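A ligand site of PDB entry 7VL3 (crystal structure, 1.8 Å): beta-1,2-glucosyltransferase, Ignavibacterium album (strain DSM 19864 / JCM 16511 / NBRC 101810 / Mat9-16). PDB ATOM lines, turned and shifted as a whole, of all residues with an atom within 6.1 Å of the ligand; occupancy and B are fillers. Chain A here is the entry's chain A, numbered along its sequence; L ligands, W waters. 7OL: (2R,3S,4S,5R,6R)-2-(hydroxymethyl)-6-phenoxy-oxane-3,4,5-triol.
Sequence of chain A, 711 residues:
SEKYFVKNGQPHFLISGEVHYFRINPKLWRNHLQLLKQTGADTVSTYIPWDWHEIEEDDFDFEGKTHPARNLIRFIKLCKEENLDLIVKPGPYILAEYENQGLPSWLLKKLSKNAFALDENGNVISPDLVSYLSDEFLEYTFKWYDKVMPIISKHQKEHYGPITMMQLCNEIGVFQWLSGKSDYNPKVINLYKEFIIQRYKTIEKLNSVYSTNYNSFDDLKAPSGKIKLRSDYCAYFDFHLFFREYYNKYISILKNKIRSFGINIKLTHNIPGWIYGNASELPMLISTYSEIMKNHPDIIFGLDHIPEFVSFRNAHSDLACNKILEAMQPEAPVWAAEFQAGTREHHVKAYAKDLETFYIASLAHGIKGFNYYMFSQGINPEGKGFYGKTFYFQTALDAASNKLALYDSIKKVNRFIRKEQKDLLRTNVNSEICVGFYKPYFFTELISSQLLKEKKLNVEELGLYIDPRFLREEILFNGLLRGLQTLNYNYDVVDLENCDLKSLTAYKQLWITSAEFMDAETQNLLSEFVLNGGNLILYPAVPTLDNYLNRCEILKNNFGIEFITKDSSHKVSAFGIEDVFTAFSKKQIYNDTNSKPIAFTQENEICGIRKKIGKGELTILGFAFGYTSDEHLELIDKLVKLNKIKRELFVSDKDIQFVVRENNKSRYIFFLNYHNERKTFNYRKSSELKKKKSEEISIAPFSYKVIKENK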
ATOM      1  N   LEU A  95     -30.488  -0.532 -22.385  1.00  0.00           N
ATOM      2  CA  LEU A  95     -29.676  -1.774 -22.484  1.00  0.00           C
ATOM      3  C   LEU A  95     -29.902  -2.583 -21.203  1.00  0.00           C
ATOM      4  O   LEU A  95     -30.950  -3.256 -21.104  1.00  0.00           O
ATOM      5  CB  LEU A  95     -28.188  -1.454 -22.682  1.00  0.00           C
ATOM      6  CG  LEU A  95     -27.725  -1.078 -24.097  1.00  0.00           C
ATOM      7  CD1 LEU A  95     -28.569   0.016 -24.710  1.00  0.00           C
ATOM      8  CD2 LEU A  95     -26.246  -0.662 -24.043  1.00  0.00           C
ATOM      9  N   GLN A 101     -33.623  -4.279 -24.941  1.00  0.00           N
ATOM     10  CA  GLN A 101     -32.781  -3.143 -24.479  1.00  0.00           C
ATOM     11  C   GLN A 101     -33.638  -2.056 -23.807  1.00  0.00           C
ATOM     12  O   GLN A 101     -33.215  -0.873 -23.801  1.00  0.00           O
ATOM     13  CB  GLN A 101     -31.999  -2.631 -25.682  1.00  0.00           C
ATOM     14  CG  GLN A 101     -31.298  -3.740 -26.463  1.00  0.00           C
ATOM     15  CD  GLN A 101     -30.159  -4.384 -25.700  1.00  0.00           C
ATOM     16  OE1 GLN A 101     -29.945  -4.101 -24.529  1.00  0.00           O
ATOM     17  NE2 GLN A 101     -29.461  -5.298 -26.350  1.00  0.00           N
ATOM     18  N   ASN A 170     -28.878   5.846 -23.723  1.00  0.00           N
ATOM     19  CA  ASN A 170     -27.833   4.994 -23.099  1.00  0.00           C
ATOM     20  C   ASN A 170     -26.779   4.627 -24.136  1.00  0.00           C
ATOM     21  O   ASN A 170     -27.159   3.982 -25.128  1.00  0.00           O
ATOM     22  CB  ASN A 170     -28.440   3.763 -22.412  1.00  0.00           C
ATOM     23  CG  ASN A 170     -27.450   3.043 -21.517  1.00  0.00           C
ATOM     24  OD1 ASN A 170     -27.287   3.369 -20.324  1.00  0.00           O
ATOM     25  ND2 ASN A 170     -26.709   2.106 -22.089  1.00  0.00           N
ATOM     26  N   GLU A 171     -25.540   5.052 -23.942  1.00  0.00           N
ATOM     27  CA  GLU A 171     -24.389   4.669 -24.839  1.00  0.00           C
ATOM     28  C   GLU A 171     -24.768   4.809 -26.331  1.00  0.00           C
ATOM     29  O   GLU A 171     -24.758   3.827 -27.101  1.00  0.00           O
ATOM     30  CB  GLU A 171     -23.977   3.248 -24.452  1.00  0.00           C
ATOM     31  CG  GLU A 171     -23.350   3.137 -23.075  1.00  0.00           C
ATOM     32  CD  GLU A 171     -22.905   1.741 -22.681  1.00  0.00           C
ATOM     33  OE1 GLU A 171     -23.367   0.781 -23.330  1.00  0.00           O
ATOM     34  OE2 GLU A 171     -22.055   1.609 -21.716  1.00  0.00           O
ATOM     35  N   VAL A 174     -23.661   2.468 -29.477  1.00  0.00           N
ATOM     36  CA  VAL A 174     -23.027   1.219 -28.971  1.00  0.00           C
ATOM     37  C   VAL A 174     -23.396   0.039 -29.896  1.00  0.00           C
ATOM     38  O   VAL A 174     -22.565  -0.821 -30.099  1.00  0.00           O
ATOM     39  CB  VAL A 174     -23.378   0.949 -27.505  1.00  0.00           C
ATOM     40  CG1 VAL A 174     -24.835   0.568 -27.295  1.00  0.00           C
ATOM     41  CG2 VAL A 174     -22.445  -0.079 -26.893  1.00  0.00           C
ATOM     42  N   PHE A 175     -24.589   0.036 -30.498  1.00  0.00           N
ATOM     43  CA  PHE A 175     -25.096  -1.022 -31.406  1.00  0.00           C
ATOM     44  C   PHE A 175     -24.427  -0.968 -32.787  1.00  0.00           C
ATOM     45  O   PHE A 175     -24.019  -2.042 -33.303  1.00  0.00           O
ATOM     46  CB  PHE A 175     -26.596  -0.855 -31.589  1.00  0.00           C
ATOM     47  CG  PHE A 175     -27.410  -0.943 -30.332  1.00  0.00           C
ATOM     48  CD1 PHE A 175     -27.518  -2.138 -29.647  1.00  0.00           C
ATOM     49  CD2 PHE A 175     -28.144   0.150 -29.882  1.00  0.00           C
ATOM     50  CE1 PHE A 175     -28.318  -2.228 -28.521  1.00  0.00           C
ATOM     51  CE2 PHE A 175     -28.951   0.054 -28.755  1.00  0.00           C
ATOM     52  CZ  PHE A 175     -29.011  -1.132 -28.060  1.00  0.00           C
ATOM     53  N   TRP A 177     -21.507   0.129 -33.190  1.00  0.00           N
ATOM     54  CA  TRP A 177     -20.104  -0.289 -32.878  1.00  0.00           C
ATOM     55  C   TRP A 177     -20.044  -1.812 -32.856  1.00  0.00           C
ATOM     56  O   TRP A 177     -19.148  -2.384 -33.540  1.00  0.00           O
ATOM     57  CB  TRP A 177     -19.635   0.269 -31.526  1.00  0.00           C
ATOM     58  CG  TRP A 177     -18.429  -0.426 -30.970  1.00  0.00           C
ATOM     59  CD1 TRP A 177     -17.277  -0.739 -31.633  1.00  0.00           C
ATOM     60  CD2 TRP A 177     -18.234  -0.869 -29.609  1.00  0.00           C
ATOM     61  NE1 TRP A 177     -16.384  -1.311 -30.759  1.00  0.00           N
ATOM     62  CE2 TRP A 177     -16.948  -1.421 -29.522  1.00  0.00           C
ATOM     63  CE3 TRP A 177     -19.032  -0.839 -28.462  1.00  0.00           C
ATOM     64  CZ2 TRP A 177     -16.438  -1.959 -28.338  1.00  0.00           C
ATOM     65  CZ3 TRP A 177     -18.529  -1.355 -27.282  1.00  0.00           C
ATOM     66  CH2 TRP A 177     -17.245  -1.909 -27.226  1.00  0.00           C
ATOM     67  N   LEU A 178     -20.913  -2.439 -32.061  1.00  0.00           N
ATOM     68  CA  LEU A 178     -20.772  -3.868 -31.728  1.00  0.00           C
ATOM     69  C   LEU A 178     -21.088  -4.713 -32.974  1.00  0.00           C
ATOM     70  O   LEU A 178     -20.530  -5.796 -33.050  1.00  0.00           O
ATOM     71  CB  LEU A 178     -21.644  -4.285 -30.537  1.00  0.00           C
ATOM     72  CG  LEU A 178     -21.198  -3.758 -29.163  1.00  0.00           C
ATOM     73  CD1 LEU A 178     -22.231  -4.091 -28.112  1.00  0.00           C
ATOM     74  CD2 LEU A 178     -19.866  -4.350 -28.717  1.00  0.00           C
ATOM     75  N   ILE A 271     -20.330   6.572 -21.649  1.00  0.00           N
ATOM     76  CA  ILE A 271     -19.384   6.143 -22.699  1.00  0.00           C
ATOM     77  C   ILE A 271     -19.106   4.643 -22.605  1.00  0.00           C
ATOM     78  O   ILE A 271     -18.486   4.198 -21.644  1.00  0.00           O
ATOM     79  CB  ILE A 271     -18.095   6.949 -22.575  1.00  0.00           C
ATOM     80  CG1 ILE A 271     -18.361   8.459 -22.597  1.00  0.00           C
ATOM     81  CG2 ILE A 271     -17.173   6.536 -23.711  1.00  0.00           C
ATOM     82  CD1 ILE A 271     -17.229   9.279 -22.007  1.00  0.00           C
ATOM     83  N   PRO A 272     -19.473   3.876 -23.645  1.00  0.00           N
ATOM     84  CA  PRO A 272     -19.106   2.467 -23.716  1.00  0.00           C
ATOM     85  C   PRO A 272     -17.661   2.314 -24.210  1.00  0.00           C
ATOM     86  O   PRO A 272     -17.043   3.293 -24.673  1.00  0.00           O
ATOM     87  CB  PRO A 272     -20.097   1.988 -24.787  1.00  0.00           C
ATOM     88  CG  PRO A 272     -20.128   3.138 -25.758  1.00  0.00           C
ATOM     89  CD  PRO A 272     -20.134   4.351 -24.862  1.00  0.00           C
ATOM     90  N   GLY A 273     -17.139   1.085 -24.217  1.00  0.00           N
ATOM     91  CA  GLY A 273     -15.882   0.783 -24.950  1.00  0.00           C
ATOM     92  C   GLY A 273     -15.051  -0.311 -24.332  1.00  0.00           C
ATOM     93  O   GLY A 273     -14.121  -0.785 -25.008  1.00  0.00           O
ATOM     94  N   TRP A 274     -15.305  -0.681 -23.090  1.00  0.00           N
ATOM     95  CA  TRP A 274     -14.557  -1.790 -22.474  1.00  0.00           C
ATOM     96  C   TRP A 274     -15.152  -3.070 -23.040  1.00  0.00           C
ATOM     97  O   TRP A 274     -16.385  -3.143 -23.192  1.00  0.00           O
ATOM     98  CB  TRP A 274     -14.683  -1.782 -20.965  1.00  0.00           C
ATOM     99  CG  TRP A 274     -13.884  -0.749 -20.247  1.00  0.00           C
ATOM    100  CD1 TRP A 274     -14.216   0.559 -20.066  1.00  0.00           C
ATOM    101  CD2 TRP A 274     -12.685  -0.972 -19.498  1.00  0.00           C
ATOM    102  NE1 TRP A 274     -13.301   1.166 -19.257  1.00  0.00           N
ATOM    103  CE2 TRP A 274     -12.358   0.263 -18.888  1.00  0.00           C
ATOM    104  CE3 TRP A 274     -11.854  -2.081 -19.273  1.00  0.00           C
ATOM    105  CZ2 TRP A 274     -11.235   0.424 -18.080  1.00  0.00           C
ATOM    106  CZ3 TRP A 274     -10.749  -1.916 -18.480  1.00  0.00           C
ATOM    107  CH2 TRP A 274     -10.464  -0.694 -17.861  1.00  0.00           C
ATOM    108  N   ILE A 275     -14.292  -4.035 -23.364  1.00  0.00           N
ATOM    109  CA  ILE A 275     -14.772  -5.418 -23.612  1.00  0.00           C
ATOM    110  C   ILE A 275     -13.629  -6.365 -23.284  1.00  0.00           C
ATOM    111  O   ILE A 275     -12.466  -5.994 -23.522  1.00  0.00           O
ATOM    112  CB  ILE A 275     -15.270  -5.542 -25.057  1.00  0.00           C
ATOM    113  CG1 ILE A 275     -16.029  -6.855 -25.258  1.00  0.00           C
ATOM    114  CG2 ILE A 275     -14.130  -5.363 -26.048  1.00  0.00           C
ATOM    115  CD1 ILE A 275     -16.679  -6.968 -26.617  1.00  0.00           C
ATOM    116  N   TYR A 276     -13.960  -7.506 -22.697  1.00  0.00           N
ATOM    117  CA  TYR A 276     -12.973  -8.504 -22.211  1.00  0.00           C
ATOM    118  C   TYR A 276     -11.918  -7.886 -21.269  1.00  0.00           C
ATOM    119  O   TYR A 276     -10.796  -8.465 -21.163  1.00  0.00           O
ATOM    120  CB  TYR A 276     -12.321  -9.180 -23.425  1.00  0.00           C
ATOM    121  CG  TYR A 276     -13.313  -9.587 -24.503  1.00  0.00           C
ATOM    122  CD1 TYR A 276     -14.428 -10.358 -24.215  1.00  0.00           C
ATOM    123  CD2 TYR A 276     -13.130  -9.207 -25.820  1.00  0.00           C
ATOM    124  CE1 TYR A 276     -15.359 -10.715 -25.185  1.00  0.00           C
ATOM    125  CE2 TYR A 276     -14.045  -9.554 -26.813  1.00  0.00           C
ATOM    126  CZ  TYR A 276     -15.161 -10.307 -26.500  1.00  0.00           C
ATOM    127  OH  TYR A 276     -16.067 -10.646 -27.463  1.00  0.00           O
ATOM    128  N   ASP A 304     -17.994   4.285 -18.596  1.00  0.00           N
ATOM    129  CA  ASP A 304     -18.532   2.961 -18.207  1.00  0.00           C
ATOM    130  C   ASP A 304     -17.359   2.002 -18.089  1.00  0.00           C
ATOM    131  O   ASP A 304     -16.955   1.425 -19.093  1.00  0.00           O
ATOM    132  CB  ASP A 304     -19.631   2.550 -19.172  1.00  0.00           C
ATOM    133  CG  ASP A 304     -20.831   3.471 -19.089  1.00  0.00           C
ATOM    134  OD1 ASP A 304     -20.948   4.212 -18.071  1.00  0.00           O
ATOM    135  OD2 ASP A 304     -21.698   3.378 -19.986  1.00  0.00           O
ATOM    136  N   ILE A 306     -15.409  -1.234 -17.113  1.00  0.00           N
ATOM    137  CA  ILE A 306     -15.646  -2.684 -16.924  1.00  0.00           C
ATOM    138  C   ILE A 306     -14.307  -3.415 -16.999  1.00  0.00           C
ATOM    139  O   ILE A 306     -14.052  -4.138 -17.968  1.00  0.00           O
ATOM    140  CB  ILE A 306     -16.655  -3.258 -17.943  1.00  0.00           C
ATOM    141  CG1 ILE A 306     -17.877  -2.360 -18.153  1.00  0.00           C
ATOM    142  CG2 ILE A 306     -17.059  -4.663 -17.511  1.00  0.00           C
ATOM    143  CD1 ILE A 306     -18.803  -2.878 -19.195  1.00  0.00           C
ATOM    144  N   GLU A 308     -13.069  -6.044 -15.204  1.00  0.00           N
ATOM    145  CA  GLU A 308     -13.258  -7.514 -14.999  1.00  0.00           C
ATOM    146  C   GLU A 308     -12.182  -8.119 -14.097  1.00  0.00           C
ATOM    147  O   GLU A 308     -12.502  -9.067 -13.383  1.00  0.00           O
ATOM    148  CB  GLU A 308     -13.362  -8.259 -16.338  1.00  0.00           C
ATOM    149  CG  GLU A 308     -14.410  -7.737 -17.315  1.00  0.00           C
ATOM    150  CD  GLU A 308     -14.588  -8.558 -18.595  1.00  0.00           C
ATOM    151  OE1 GLU A 308     -13.775  -9.491 -18.827  1.00  0.00           O
ATOM    152  OE2 GLU A 308     -15.489  -8.249 -19.388  1.00  0.00           O
ATOM    153  N   GLU A 338     -20.846   4.321 -14.765  1.00  0.00           N
ATOM    154  CA  GLU A 338     -20.987   2.903 -14.417  1.00  0.00           C
ATOM    155  C   GLU A 338     -19.589   2.457 -14.014  1.00  0.00           C
ATOM    156  O   GLU A 338     -18.684   2.551 -14.863  1.00  0.00           O
ATOM    157  CB  GLU A 338     -21.531   2.077 -15.587  1.00  0.00           C
ATOM    158  CG  GLU A 338     -22.898   2.537 -16.090  1.00  0.00           C
ATOM    159  CD  GLU A 338     -23.341   1.854 -17.388  1.00  0.00           C
ATOM    160  OE1 GLU A 338     -22.821   0.784 -17.713  1.00  0.00           O
ATOM    161  OE2 GLU A 338     -24.168   2.417 -18.103  1.00  0.00           O
ATOM    162  N   ARG A 344     -21.575  -8.595 -14.687  1.00  0.00           N
ATOM    163  CA  ARG A 344     -22.767  -8.803 -15.527  1.00  0.00           C
ATOM    164  C   ARG A 344     -22.824 -10.256 -16.018  1.00  0.00           C
ATOM    165  O   ARG A 344     -23.899 -10.637 -16.469  1.00  0.00           O
ATOM    166  CB  ARG A 344     -22.715  -7.839 -16.712  1.00  0.00           C
ATOM    167  CG  ARG A 344     -21.453  -8.039 -17.543  1.00  0.00           C
ATOM    168  CD  ARG A 344     -21.404  -7.067 -18.684  1.00  0.00           C
ATOM    169  NE  ARG A 344     -20.197  -7.219 -19.481  1.00  0.00           N
ATOM    170  CZ  ARG A 344     -19.950  -6.546 -20.593  1.00  0.00           C
ATOM    171  NH1 ARG A 344     -18.843  -6.784 -21.263  1.00  0.00           N
ATOM    172  NH2 ARG A 344     -20.827  -5.678 -21.039  1.00  0.00           N
ATOM    173  N   TYR A 387     -30.779 -12.480 -20.767  1.00  0.00           N
ATOM    174  CA  TYR A 387     -29.782 -13.587 -20.765  1.00  0.00           C
ATOM    175  C   TYR A 387     -30.006 -14.639 -19.665  1.00  0.00           C
ATOM    176  O   TYR A 387     -29.242 -15.639 -19.644  1.00  0.00           O
ATOM    177  CB  TYR A 387     -28.388 -13.038 -20.475  1.00  0.00           C
ATOM    178  CG  TYR A 387     -27.707 -12.334 -21.615  1.00  0.00           C
ATOM    179  CD1 TYR A 387     -27.391 -12.984 -22.798  1.00  0.00           C
ATOM    180  CD2 TYR A 387     -27.276 -11.012 -21.460  1.00  0.00           C
ATOM    181  CE1 TYR A 387     -26.735 -12.331 -23.835  1.00  0.00           C
ATOM    182  CE2 TYR A 387     -26.598 -10.351 -22.471  1.00  0.00           C
ATOM    183  CZ  TYR A 387     -26.317 -11.020 -23.647  1.00  0.00           C
ATOM    184  OH  TYR A 387     -25.653 -10.355 -24.632  1.00  0.00           O
HETATM  185  O6  7OL L   1     -18.398  -4.964 -23.420  1.00  0.00           O
HETATM  186  C6  7OL L   1     -19.052  -4.418 -24.594  1.00  0.00           C
HETATM  187  C4  7OL L   1     -20.064  -3.363 -24.138  1.00  0.00           C
HETATM  188  C2  7OL L   1     -19.501  -2.316 -23.186  1.00  0.00           C
HETATM  189  O3  7OL L   1     -18.470  -1.584 -23.858  1.00  0.00           O
HETATM  190  C1  7OL L   1     -20.644  -1.337 -22.824  1.00  0.00           C
HETATM  191  O2  7OL L   1     -20.156  -0.399 -21.870  1.00  0.00           O
HETATM  192  C3  7OL L   1     -21.801  -2.126 -22.180  1.00  0.00           C
HETATM  193  O5  7OL L   1     -22.908  -1.253 -21.890  1.00  0.00           O
HETATM  194  C5  7OL L   1     -22.224  -3.288 -23.066  1.00  0.00           C
HETATM  195  O1  7OL L   1     -21.110  -4.078 -23.470  1.00  0.00           O
HETATM  196  O4  7OL L   1     -22.856  -2.841 -24.254  1.00  0.00           O
HETATM  197  C7  7OL L   1     -23.710  -3.678 -24.953  1.00  0.00           C
HETATM  198  C9  7OL L   1     -24.563  -3.095 -25.868  1.00  0.00           C
HETATM  199  C11 7OL L   1     -25.459  -3.907 -26.614  1.00  0.00           C
HETATM  200  C12 7OL L   1     -25.499  -5.296 -26.488  1.00  0.00           C
HETATM  201  C10 7OL L   1     -24.617  -5.896 -25.574  1.00  0.00           C
HETATM  202  C8  7OL L   1     -23.746  -5.085 -24.810  1.00  0.00           C
HETATM  203  O   HOH W   1     -22.849  -1.667 -19.056  1.00  0.00           O
HETATM  204  O   HOH W   2     -17.463  -0.053 -21.265  1.00  0.00           O
HETATM  205  O   HOH W   3     -25.359  -3.170 -21.247  1.00  0.00           O
HETATM  206  O   HOH W   4     -24.498   0.846 -20.309  1.00  0.00           O
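An oxygen (O5) of the ligand lies within hydrogen-bond range of the side-chain carboxylate of Glu 171. N of Trp 274 sits at hydrogen-bond distance from O3 of the ligand (3.4 Å). O of Trp 274 sits at hydrogen-bond distance from O3 of the ligand, 2.7 Å away. The guanidinium group of Arg 344 sits at hydrogen-bond distance from an oxygen (O6) of the ligand (2.9 Å). An oxygen (O3) of the ligand sits at hydrogen-bond distance from the backbone NH of Gly 273, 3.0 Å away.
The side-chain carboxylate (OD2) of Asp 304 lies close to the side-chain carboxylate (OE2) of Glu 171 (2.5 Å). The backbone NH (N) of Leu 95 sits at hydrogen-bond distance from the backbone carbonyl oxygen (O) of Gln 101.
Residues that only touch the ligand: Leu 178, Trp 177, Leu 95, Ile 275, Pro 272, Phe 175, Val 174, Ile 306 and Gln 101. Hydrophobic or aromatic side chains that line the ligand: Leu 95, Val 174, Phe 175, Trp 177, Leu 178, Pro 272, Ile 275 and Ile 306. The nearest printed residue that does not touch the ligand is Asp 304 (4.03 Å).
Water W2 lies within hydrogen-bond range of the backbone carbonyl oxygen of Asp 304 (2.7 Å), an oxygen (O2) of the ligand (2.8 Å), the backbone NH of Trp 274 (2.9 Å) and the backbone NH of Gly 273 (3.2 Å). Water W1 lies within hydrogen-bond range of OE1 of Glu 338 (2.8 Å) and O5 of the ligand (2.9 Å). Water W4 lies within hydrogen-bond range of OE2 of Glu 338 (2.7 Å), OE2 of Glu 171 (2.9 Å), O5 of the ligand (3.1 Å) and ND2 of Asn 170 (3.1 Å).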
